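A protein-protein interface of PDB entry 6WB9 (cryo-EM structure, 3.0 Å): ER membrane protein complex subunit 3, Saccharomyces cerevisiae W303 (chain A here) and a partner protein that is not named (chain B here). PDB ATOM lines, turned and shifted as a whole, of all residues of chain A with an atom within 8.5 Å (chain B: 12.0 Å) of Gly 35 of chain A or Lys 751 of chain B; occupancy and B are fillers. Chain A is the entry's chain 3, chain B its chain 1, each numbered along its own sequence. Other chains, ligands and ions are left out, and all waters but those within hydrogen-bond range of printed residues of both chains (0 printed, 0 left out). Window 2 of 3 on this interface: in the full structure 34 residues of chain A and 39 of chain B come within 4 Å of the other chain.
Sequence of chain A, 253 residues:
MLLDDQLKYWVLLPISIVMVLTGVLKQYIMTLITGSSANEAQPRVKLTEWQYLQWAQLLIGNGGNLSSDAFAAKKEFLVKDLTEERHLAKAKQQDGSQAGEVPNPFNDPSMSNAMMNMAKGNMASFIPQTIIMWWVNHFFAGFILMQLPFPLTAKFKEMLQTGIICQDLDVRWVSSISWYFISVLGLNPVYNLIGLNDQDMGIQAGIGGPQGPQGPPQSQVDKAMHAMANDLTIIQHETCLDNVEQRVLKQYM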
ATOM      1  N   TYR A  28      -1.807  -4.481 -20.490  1.00  0.00           N
ATOM      2  CA  TYR A  28      -1.565  -3.201 -21.151  1.00  0.00           C
ATOM      3  C   TYR A  28      -2.710  -2.221 -20.908  1.00  0.00           C
ATOM      4  O   TYR A  28      -2.475  -1.027 -20.680  1.00  0.00           O
ATOM      5  CB  TYR A  28      -1.345  -3.421 -22.649  1.00  0.00           C
ATOM      6  CG  TYR A  28       0.013  -3.997 -23.018  1.00  0.00           C
ATOM      7  CD1 TYR A  28       0.995  -4.208 -22.057  1.00  0.00           C
ATOM      8  CD2 TYR A  28       0.313  -4.316 -24.335  1.00  0.00           C
ATOM      9  CE1 TYR A  28       2.227  -4.733 -22.398  1.00  0.00           C
ATOM     10  CE2 TYR A  28       1.543  -4.830 -24.686  1.00  0.00           C
ATOM     11  CZ  TYR A  28       2.494  -5.040 -23.714  1.00  0.00           C
ATOM     12  OH  TYR A  28       3.720  -5.558 -24.058  1.00  0.00           O
ATOM     13  N   ILE A  29      -3.950  -2.715 -20.917  1.00  0.00           N
ATOM     14  CA  ILE A  29      -5.109  -1.874 -20.639  1.00  0.00           C
ATOM     15  C   ILE A  29      -5.114  -1.429 -19.181  1.00  0.00           C
ATOM     16  O   ILE A  29      -5.384  -0.262 -18.882  1.00  0.00           O
ATOM     17  CB  ILE A  29      -6.402  -2.618 -21.037  1.00  0.00           C
ATOM     18  CG1 ILE A  29      -6.587  -2.594 -22.555  1.00  0.00           C
ATOM     19  CG2 ILE A  29      -7.639  -2.032 -20.365  1.00  0.00           C
ATOM     20  CD1 ILE A  29      -6.696  -1.210 -23.133  1.00  0.00           C
ATOM     21  N   MET A  30      -4.764  -2.323 -18.252  1.00  0.00           N
ATOM     22  CA  MET A  30      -4.722  -1.929 -16.851  1.00  0.00           C
ATOM     23  C   MET A  30      -3.507  -1.078 -16.503  1.00  0.00           C
ATOM     24  O   MET A  30      -3.494  -0.468 -15.430  1.00  0.00           O
ATOM     25  CB  MET A  30      -4.766  -3.164 -15.948  1.00  0.00           C
ATOM     26  CG  MET A  30      -6.120  -3.856 -15.918  1.00  0.00           C
ATOM     27  SD  MET A  30      -7.467  -2.759 -15.436  1.00  0.00           S
ATOM     28  CE  MET A  30      -7.090  -2.499 -13.706  1.00  0.00           C
ATOM     29  N   THR A  31      -2.488  -1.021 -17.364  1.00  0.00           N
ATOM     30  CA  THR A  31      -1.467   0.007 -17.176  1.00  0.00           C
ATOM     31  C   THR A  31      -1.910   1.346 -17.754  1.00  0.00           C
ATOM     32  O   THR A  31      -1.650   2.392 -17.153  1.00  0.00           O
ATOM     33  CB  THR A  31      -0.136  -0.412 -17.800  1.00  0.00           C
ATOM     34  OG1 THR A  31      -0.352  -0.868 -19.138  1.00  0.00           O
ATOM     35  CG2 THR A  31       0.530  -1.504 -16.980  1.00  0.00           C
ATOM     36  N   LEU A  32      -2.573   1.337 -18.917  1.00  0.00           N
ATOM     37  CA  LEU A  32      -2.979   2.594 -19.545  1.00  0.00           C
ATOM     38  C   LEU A  32      -4.127   3.270 -18.804  1.00  0.00           C
ATOM     39  O   LEU A  32      -4.187   4.503 -18.755  1.00  0.00           O
ATOM     40  CB  LEU A  32      -3.377   2.358 -21.000  1.00  0.00           C
ATOM     41  CG  LEU A  32      -2.244   2.157 -22.002  1.00  0.00           C
ATOM     42  CD1 LEU A  32      -2.806   1.954 -23.392  1.00  0.00           C
ATOM     43  CD2 LEU A  32      -1.304   3.341 -21.975  1.00  0.00           C
ATOM     44  N   ILE A  33      -5.044   2.490 -18.234  1.00  0.00           N
ATOM     45  CA  ILE A  33      -6.195   3.060 -17.540  1.00  0.00           C
ATOM     46  C   ILE A  33      -5.789   3.580 -16.168  1.00  0.00           C
ATOM     47  O   ILE A  33      -6.079   4.728 -15.812  1.00  0.00           O
ATOM     48  CB  ILE A  33      -7.326   2.018 -17.446  1.00  0.00           C
ATOM     49  CG1 ILE A  33      -7.960   1.791 -18.818  1.00  0.00           C
ATOM     50  CG2 ILE A  33      -8.385   2.449 -16.446  1.00  0.00           C
ATOM     51  CD1 ILE A  33      -8.567   3.035 -19.421  1.00  0.00           C
ATOM     52  N   THR A  34      -5.097   2.752 -15.384  1.00  0.00           N
ATOM     53  CA  THR A  34      -4.645   3.142 -14.050  1.00  0.00           C
ATOM     54  C   THR A  34      -3.460   4.091 -14.202  1.00  0.00           C
ATOM     55  O   THR A  34      -2.290   3.704 -14.162  1.00  0.00           O
ATOM     56  CB  THR A  34      -4.276   1.918 -13.221  1.00  0.00           C
ATOM     57  OG1 THR A  34      -5.318   0.939 -13.323  1.00  0.00           O
ATOM     58  CG2 THR A  34      -4.097   2.297 -11.757  1.00  0.00           C
ATOM     59  N   GLY A  35      -3.781   5.370 -14.396  1.00  0.00           N
ATOM     60  CA  GLY A  35      -2.775   6.405 -14.492  1.00  0.00           C
ATOM     61  C   GLY A  35      -2.342   6.992 -13.174  1.00  0.00           C
ATOM     62  O   GLY A  35      -1.369   7.750 -13.131  1.00  0.00           O
ATOM     63  N   SER A  36      -3.047   6.662 -12.097  1.00  0.00           N
ATOM     64  CA  SER A  36      -2.697   7.165 -10.780  1.00  0.00           C
ATOM     65  C   SER A  36      -1.437   6.479 -10.258  1.00  0.00           C
ATOM     66  O   SER A  36      -1.086   5.365 -10.654  1.00  0.00           O
ATOM     67  CB  SER A  36      -3.854   6.958  -9.802  1.00  0.00           C
ATOM     68  OG  SER A  36      -4.174   5.584  -9.672  1.00  0.00           O
ATOM     69  N   SER A  37      -0.753   7.172  -9.351  1.00  0.00           N
ATOM     70  CA  SER A  37       0.469   6.665  -8.744  1.00  0.00           C
ATOM     71  C   SER A  37       0.345   6.711  -7.228  1.00  0.00           C
ATOM     72  O   SER A  37      -0.755   6.905  -6.700  1.00  0.00           O
ATOM     73  CB  SER A  37       1.682   7.472  -9.211  1.00  0.00           C
ATOM     74  OG  SER A  37       1.595   8.817  -8.775  1.00  0.00           O
ATOM     75  N   ALA A  38       1.464   6.508  -6.522  1.00  0.00           N
ATOM     76  CA  ALA A  38       1.466   6.656  -5.070  1.00  0.00           C
ATOM     77  C   ALA A  38       1.192   8.095  -4.650  1.00  0.00           C
ATOM     78  O   ALA A  38       0.634   8.330  -3.572  1.00  0.00           O
ATOM     79  CB  ALA A  38       2.800   6.179  -4.495  1.00  0.00           C
ATOM     80  N   ASN A  39       1.571   9.061  -5.481  1.00  0.00           N
ATOM     81  CA  ASN A  39       1.217  10.457  -5.289  1.00  0.00           C
ATOM     82  C   ASN A  39       0.063  10.835  -6.214  1.00  0.00           C
ATOM     83  O   ASN A  39      -0.332  10.078  -7.103  1.00  0.00           O
ATOM     84  CB  ASN A  39       2.427  11.361  -5.548  1.00  0.00           C
ATOM     85  CG  ASN A  39       3.673  10.887  -4.828  1.00  0.00           C
ATOM     86  OD1 ASN A  39       3.597  10.127  -3.863  1.00  0.00           O
ATOM     87  ND2 ASN A  39       4.832  11.338  -5.296  1.00  0.00           N
ATOM     88  N   GLU A  40      -0.482  12.027  -5.989  1.00  0.00           N
ATOM     89  CA  GLU A  40      -1.561  12.575  -6.799  1.00  0.00           C
ATOM     90  C   GLU A  40      -1.181  13.983  -7.245  1.00  0.00           C
ATOM     91  O   GLU A  40      -0.113  14.499  -6.906  1.00  0.00           O
ATOM     92  CB  GLU A  40      -2.889  12.588  -6.030  1.00  0.00           C
ATOM     93  CG  GLU A  40      -3.438  11.211  -5.692  1.00  0.00           C
ATOM     94  CD  GLU A  40      -4.788  11.277  -5.005  1.00  0.00           C
ATOM     95  OE1 GLU A  40      -5.333  12.393  -4.867  1.00  0.00           O
ATOM     96  OE2 GLU A  40      -5.306  10.214  -4.603  1.00  0.00           O
ATOM     97  N   PHE B 743       0.145  -2.560 -31.677  1.00  0.00           N
ATOM     98  CA  PHE B 743      -0.127  -1.132 -31.770  1.00  0.00           C
ATOM     99  C   PHE B 743      -0.279  -0.464 -30.410  1.00  0.00           C
ATOM    100  O   PHE B 743       0.003   0.733 -30.288  1.00  0.00           O
ATOM    101  CB  PHE B 743      -1.387  -0.883 -32.603  1.00  0.00           C
ATOM    102  CG  PHE B 743      -1.180  -1.051 -34.084  1.00  0.00           C
ATOM    103  CD1 PHE B 743       0.098  -1.068 -34.626  1.00  0.00           C
ATOM    104  CD2 PHE B 743      -2.267  -1.185 -34.935  1.00  0.00           C
ATOM    105  CE1 PHE B 743       0.289  -1.221 -35.984  1.00  0.00           C
ATOM    106  CE2 PHE B 743      -2.083  -1.338 -36.297  1.00  0.00           C
ATOM    107  CZ  PHE B 743      -0.803  -1.356 -36.820  1.00  0.00           C
ATOM    108  N   ILE B 744      -0.718  -1.200 -29.384  1.00  0.00           N
ATOM    109  CA  ILE B 744      -0.884  -0.613 -28.058  1.00  0.00           C
ATOM    110  C   ILE B 744       0.370  -0.749 -27.204  1.00  0.00           C
ATOM    111  O   ILE B 744       0.463  -0.093 -26.154  1.00  0.00           O
ATOM    112  CB  ILE B 744      -2.119  -1.236 -27.368  1.00  0.00           C
ATOM    113  CG1 ILE B 744      -2.791  -0.231 -26.435  1.00  0.00           C
ATOM    114  CG2 ILE B 744      -1.760  -2.497 -26.607  1.00  0.00           C
ATOM    115  CD1 ILE B 744      -4.016  -0.776 -25.745  1.00  0.00           C
ATOM    116  N   ARG B 745       1.343  -1.560 -27.625  1.00  0.00           N
ATOM    117  CA  ARG B 745       2.596  -1.669 -26.879  1.00  0.00           C
ATOM    118  C   ARG B 745       3.436  -0.384 -26.827  1.00  0.00           C
ATOM    119  O   ARG B 745       3.939  -0.074 -25.731  1.00  0.00           O
ATOM    120  CB  ARG B 745       3.397  -2.866 -27.424  1.00  0.00           C
ATOM    121  CG  ARG B 745       4.895  -2.799 -27.199  1.00  0.00           C
ATOM    122  CD  ARG B 745       5.565  -4.129 -27.481  1.00  0.00           C
ATOM    123  NE  ARG B 745       7.018  -4.024 -27.394  1.00  0.00           N
ATOM    124  CZ  ARG B 745       7.711  -4.119 -26.264  1.00  0.00           C
ATOM    125  NH1 ARG B 745       7.087  -4.326 -25.112  1.00  0.00           N
ATOM    126  NH2 ARG B 745       9.032  -4.008 -26.286  1.00  0.00           N
ATOM    127  N   PRO B 746       3.632   0.402 -27.907  1.00  0.00           N
ATOM    128  CA  PRO B 746       4.348   1.679 -27.719  1.00  0.00           C
ATOM    129  C   PRO B 746       3.587   2.701 -26.891  1.00  0.00           C
ATOM    130  O   PRO B 746       4.224   3.560 -26.271  1.00  0.00           O
ATOM    131  CB  PRO B 746       4.578   2.178 -29.152  1.00  0.00           C
ATOM    132  CG  PRO B 746       3.556   1.504 -29.952  1.00  0.00           C
ATOM    133  CD  PRO B 746       3.459   0.146 -29.353  1.00  0.00           C
ATOM    134  N   SER B 747       2.257   2.615 -26.828  1.00  0.00           N
ATOM    135  CA  SER B 747       1.500   3.493 -25.940  1.00  0.00           C
ATOM    136  C   SER B 747       1.786   3.183 -24.475  1.00  0.00           C
ATOM    137  O   SER B 747       1.916   4.099 -23.656  1.00  0.00           O
ATOM    138  CB  SER B 747       0.006   3.369 -26.231  1.00  0.00           C
ATOM    139  OG  SER B 747      -0.747   4.210 -25.378  1.00  0.00           O
ATOM    140  N   VAL B 748       1.932   1.901 -24.135  1.00  0.00           N
ATOM    141  CA  VAL B 748       2.283   1.521 -22.769  1.00  0.00           C
ATOM    142  C   VAL B 748       3.739   1.867 -22.478  1.00  0.00           C
ATOM    143  O   VAL B 748       4.071   2.348 -21.386  1.00  0.00           O
ATOM    144  CB  VAL B 748       1.992   0.026 -22.547  1.00  0.00           C
ATOM    145  CG1 VAL B 748       2.341  -0.398 -21.131  1.00  0.00           C
ATOM    146  CG2 VAL B 748       0.539  -0.254 -22.825  1.00  0.00           C
ATOM    147  N   SER B 749       4.626   1.649 -23.455  1.00  0.00           N
ATOM    148  CA  SER B 749       6.034   1.996 -23.291  1.00  0.00           C
ATOM    149  C   SER B 749       6.260   3.498 -23.186  1.00  0.00           C
ATOM    150  O   SER B 749       7.276   3.920 -22.626  1.00  0.00           O
ATOM    151  CB  SER B 749       6.849   1.434 -24.454  1.00  0.00           C
ATOM    152  OG  SER B 749       8.183   1.906 -24.410  1.00  0.00           O
ATOM    153  N   ASN B 750       5.343   4.310 -23.711  1.00  0.00           N
ATOM    154  CA  ASN B 750       5.396   5.752 -23.526  1.00  0.00           C
ATOM    155  C   ASN B 750       4.724   6.199 -22.236  1.00  0.00           C
ATOM    156  O   ASN B 750       5.186   7.157 -21.606  1.00  0.00           O
ATOM    157  CB  ASN B 750       4.747   6.453 -24.723  1.00  0.00           C
ATOM    158  CG  ASN B 750       4.822   7.960 -24.628  1.00  0.00           C
ATOM    159  OD1 ASN B 750       5.862   8.559 -24.900  1.00  0.00           O
ATOM    160  ND2 ASN B 750       3.714   8.584 -24.251  1.00  0.00           N
ATOM    161  N   LYS B 751       3.658   5.514 -21.810  1.00  0.00           N
ATOM    162  CA  LYS B 751       2.981   5.906 -20.580  1.00  0.00           C
ATOM    163  C   LYS B 751       3.800   5.555 -19.344  1.00  0.00           C
ATOM    164  O   LYS B 751       3.783   6.305 -18.361  1.00  0.00           O
ATOM    165  CB  LYS B 751       1.606   5.252 -20.499  1.00  0.00           C
ATOM    166  CG  LYS B 751       0.688   5.910 -19.493  1.00  0.00           C
ATOM    167  CD  LYS B 751       0.106   4.899 -18.533  1.00  0.00           C
ATOM    168  CE  LYS B 751      -0.825   5.572 -17.546  1.00  0.00           C
ATOM    169  NZ  LYS B 751      -0.113   6.579 -16.716  1.00  0.00           N
ATOM    170  N   LYS B 752       4.533   4.436 -19.376  1.00  0.00           N
ATOM    171  CA  LYS B 752       5.428   4.117 -18.265  1.00  0.00           C
ATOM    172  C   LYS B 752       6.588   5.102 -18.193  1.00  0.00           C
ATOM    173  O   LYS B 752       7.032   5.467 -17.099  1.00  0.00           O
ATOM    174  CB  LYS B 752       5.948   2.687 -18.395  1.00  0.00           C
ATOM    175  CG  LYS B 752       4.882   1.617 -18.243  1.00  0.00           C
ATOM    176  CD  LYS B 752       5.501   0.234 -18.141  1.00  0.00           C
ATOM    177  CE  LYS B 752       6.395  -0.070 -19.332  1.00  0.00           C
ATOM    178  NZ  LYS B 752       7.100  -1.370 -19.172  1.00  0.00           N
ATOM    179  N   LEU B 753       7.064   5.570 -19.348  1.00  0.00           N
ATOM    180  CA  LEU B 753       8.117   6.579 -19.372  1.00  0.00           C
ATOM    181  C   LEU B 753       7.611   7.921 -18.854  1.00  0.00           C
ATOM    182  O   LEU B 753       8.339   8.642 -18.159  1.00  0.00           O
ATOM    183  CB  LEU B 753       8.659   6.716 -20.791  1.00  0.00           C
ATOM    184  CG  LEU B 753       9.820   7.678 -21.008  1.00  0.00           C
ATOM    185  CD1 LEU B 753      11.029   7.209 -20.247  1.00  0.00           C
ATOM    186  CD2 LEU B 753      10.132   7.780 -22.478  1.00  0.00           C
ATOM    187  N   LYS B 754       6.361   8.264 -19.175  1.00  0.00           N
ATOM    188  CA  LYS B 754       5.757   9.477 -18.630  1.00  0.00           C
ATOM    189  C   LYS B 754       5.537   9.361 -17.127  1.00  0.00           C
ATOM    190  O   LYS B 754       5.651  10.353 -16.402  1.00  0.00           O
ATOM    191  CB  LYS B 754       4.437   9.769 -19.338  1.00  0.00           C
ATOM    192  CG  LYS B 754       4.583  10.339 -20.734  1.00  0.00           C
ATOM    193  CD  LYS B 754       3.235  10.442 -21.433  1.00  0.00           C
ATOM    194  CE  LYS B 754       2.231  11.256 -20.626  1.00  0.00           C
ATOM    195  NZ  LYS B 754       1.191  10.396 -19.992  1.00  0.00           N
ATOM    196  N   SER B 755       5.216   8.160 -16.642  1.00  0.00           N
ATOM    197  CA  SER B 755       5.122   7.953 -15.201  1.00  0.00           C
ATOM    198  C   SER B 755       6.486   8.052 -14.531  1.00  0.00           C
ATOM    199  O   SER B 755       6.581   8.494 -13.381  1.00  0.00           O
ATOM    200  CB  SER B 755       4.483   6.597 -14.908  1.00  0.00           C
ATOM    201  OG  SER B 755       4.500   6.314 -13.521  1.00  0.00           O
ATOM    202  N   GLN B 756       7.548   7.648 -15.231  1.00  0.00           N
ATOM    203  CA  GLN B 756       8.890   7.773 -14.675  1.00  0.00           C
ATOM    204  C   GLN B 756       9.370   9.219 -14.660  1.00  0.00           C
ATOM    205  O   GLN B 756      10.137   9.601 -13.768  1.00  0.00           O
ATOM    206  CB  GLN B 756       9.876   6.913 -15.461  1.00  0.00           C
ATOM    207  CG  GLN B 756       9.735   5.425 -15.230  1.00  0.00           C
ATOM    208  CD  GLN B 756      10.773   4.625 -15.981  1.00  0.00           C
ATOM    209  OE1 GLN B 756      11.968   4.747 -15.726  1.00  0.00           O
ATOM    210  NE2 GLN B 756      10.322   3.804 -16.922  1.00  0.00           N
ATOM    211  N   TRP B 757       8.947  10.034 -15.624  1.00  0.00           N
ATOM    212  CA  TRP B 757       9.487  11.385 -15.754  1.00  0.00           C
ATOM    213  C   TRP B 757       8.572  12.473 -15.207  1.00  0.00           C
ATOM    214  O   TRP B 757       9.038  13.333 -14.455  1.00  0.00           O
ATOM    215  CB  TRP B 757       9.821  11.676 -17.218  1.00  0.00           C
ATOM    216  CG  TRP B 757      11.130  11.111 -17.632  1.00  0.00           C
ATOM    217  CD1 TRP B 757      11.421   9.800 -17.843  1.00  0.00           C
ATOM    218  CD2 TRP B 757      12.336  11.836 -17.883  1.00  0.00           C
ATOM    219  NE1 TRP B 757      12.734   9.660 -18.213  1.00  0.00           N
ATOM    220  CE2 TRP B 757      13.318  10.899 -18.247  1.00  0.00           C
ATOM    221  CE3 TRP B 757      12.680  13.188 -17.843  1.00  0.00           C
ATOM    222  CZ2 TRP B 757      14.621  11.268 -18.562  1.00  0.00           C
ATOM    223  CZ3 TRP B 757      13.973  13.551 -18.162  1.00  0.00           C
ATOM    224  CH2 TRP B 757      14.927  12.598 -18.513  1.00  0.00           C
ATOM    225  N   LEU B 758       7.286  12.474 -15.578  1.00  0.00           N
ATOM    226  CA  LEU B 758       6.404  13.568 -15.168  1.00  0.00           C
ATOM    227  C   LEU B 758       6.095  13.504 -13.679  1.00  0.00           C
ATOM    228  O   LEU B 758       6.065  14.538 -13.002  1.00  0.00           O
ATOM    229  CB  LEU B 758       5.096  13.550 -15.968  1.00  0.00           C
ATOM    230  CG  LEU B 758       5.049  13.434 -17.495  1.00  0.00           C
ATOM    231  CD1 LEU B 758       3.614  13.578 -17.963  1.00  0.00           C
ATOM    232  CD2 LEU B 758       5.926  14.448 -18.186  1.00  0.00           C
ATOM    233  N   ILE B 759       5.865  12.307 -13.153  1.00  0.00           N
ATOM    234  CA  ILE B 759       5.545  12.144 -11.744  1.00  0.00           C
ATOM    235  C   ILE B 759       6.827  12.085 -10.927  1.00  0.00           C
ATOM    236  O   ILE B 759       7.558  13.069 -10.837  1.00  0.00           O
ATOM    237  CB  ILE B 759       4.683  10.890 -11.509  1.00  0.00           C
ATOM    238  CG1 ILE B 759       3.445  10.918 -12.410  1.00  0.00           C
ATOM    239  CG2 ILE B 759       4.281  10.786 -10.045  1.00  0.00           C
ATOM    240  CD1 ILE B 759       2.573   9.687 -12.295  1.00  0.00           C
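Gly 35 of chain A touches just one residue of chain B: Lys 751 (3.5 Å).
Of chain A, only Thr 31 (3.3 Å), Leu 32 (3.7 Å) and Gly 35 (3.5 Å) come within 4 Å of Lys 751 of chain B.
Of the printed residues of chain B, Thr 31 of chain A touches Val 748 and Lys 751.
Leu 32 of chain A touches four residues of chain B.
No residue of chain B comes within 4 Å of Ile 33 of chain A.
Thr 34 of chain A touches none of the printed residues of chain B.
No residue of chain B comes within 4 Å of Ser 36 of chain A.
Ser 37 of chain A touches one residue of chain B.
Printed residues of chain A within 4 Å of Arg 745 of chain B: Tyr 28.
Of the printed residues of chain A, Val 748 of chain B touches Tyr 28, Thr 31 and Leu 32.
Printed residues of chain A within 4 Å of Ser 747 of chain B: Leu 32.
Printed residues of chain B within 4 Å of Tyr 28 of chain A: Ile 744 (3.6 Å), Arg 745 (3.7 Å) and Val 748 (3.7 Å).
Asn 750 of chain B touches none of the printed residues of chain A.
Pro 746 of chain B touches none of the printed residues of chain A.
The nearest residue of chain A that does not touch Lys 751 of chain B is Thr 34 of chain A (4.1 Å).
Among the printed residues, merely in contact across the chains: Tyr 28 of chain A with Ile 744 of chain B, Tyr 28 of chain A with Arg 745 of chain B, Tyr 28 of chain A with Val 748 of chain B, Ile 29 of chain A with Ile 744 of chain B, Thr 31 of chain A with Val 748 of chain B, Thr 31 of chain A with Lys 751 of chain B, Leu 32 of chain A with Ile 744 of chain B, Leu 32 of chain A with Ser 747 of chain B, Leu 32 of chain A with Val 748 of chain B, Leu 32 of chain A with Lys 751 of chain B, Gly 35 of chain A with Lys 751 of chain B and Ser 37 of chain A with Ile 759 of chain B.
The backbone carbonyl oxygen of Asn 39 of chain A sits at hydrogen-bond distance from the side-chain hydroxyl of Ser 37 of chain A (2.8 Å).
The backbone carbonyl oxygen of Tyr 28 of chain A lies within hydrogen-bond range of the side-chain hydroxyl of Thr 31 of chain A, at 2.6 Å.
Hydrophobic or aromatic side chains of chain B that line the printed part of chain A: Ile 744, Val 748 and Ile 759.
Printed residues of chain A that touch a printed residue of chain B: Tyr 28, Ile 29, Thr 31, Leu 32, Gly 35 and Ser 37.
Hydrophobic or aromatic side chains of chain A that line the printed part of chain B: Tyr 28, Ile 29 and Leu 32.
Among the printed residues, 12 pairs touch across the chains.
Among the printed residues, no Asp or Glu carboxylate lies within 4 Å of a Lys or Arg side-chain nitrogen of the other chain.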
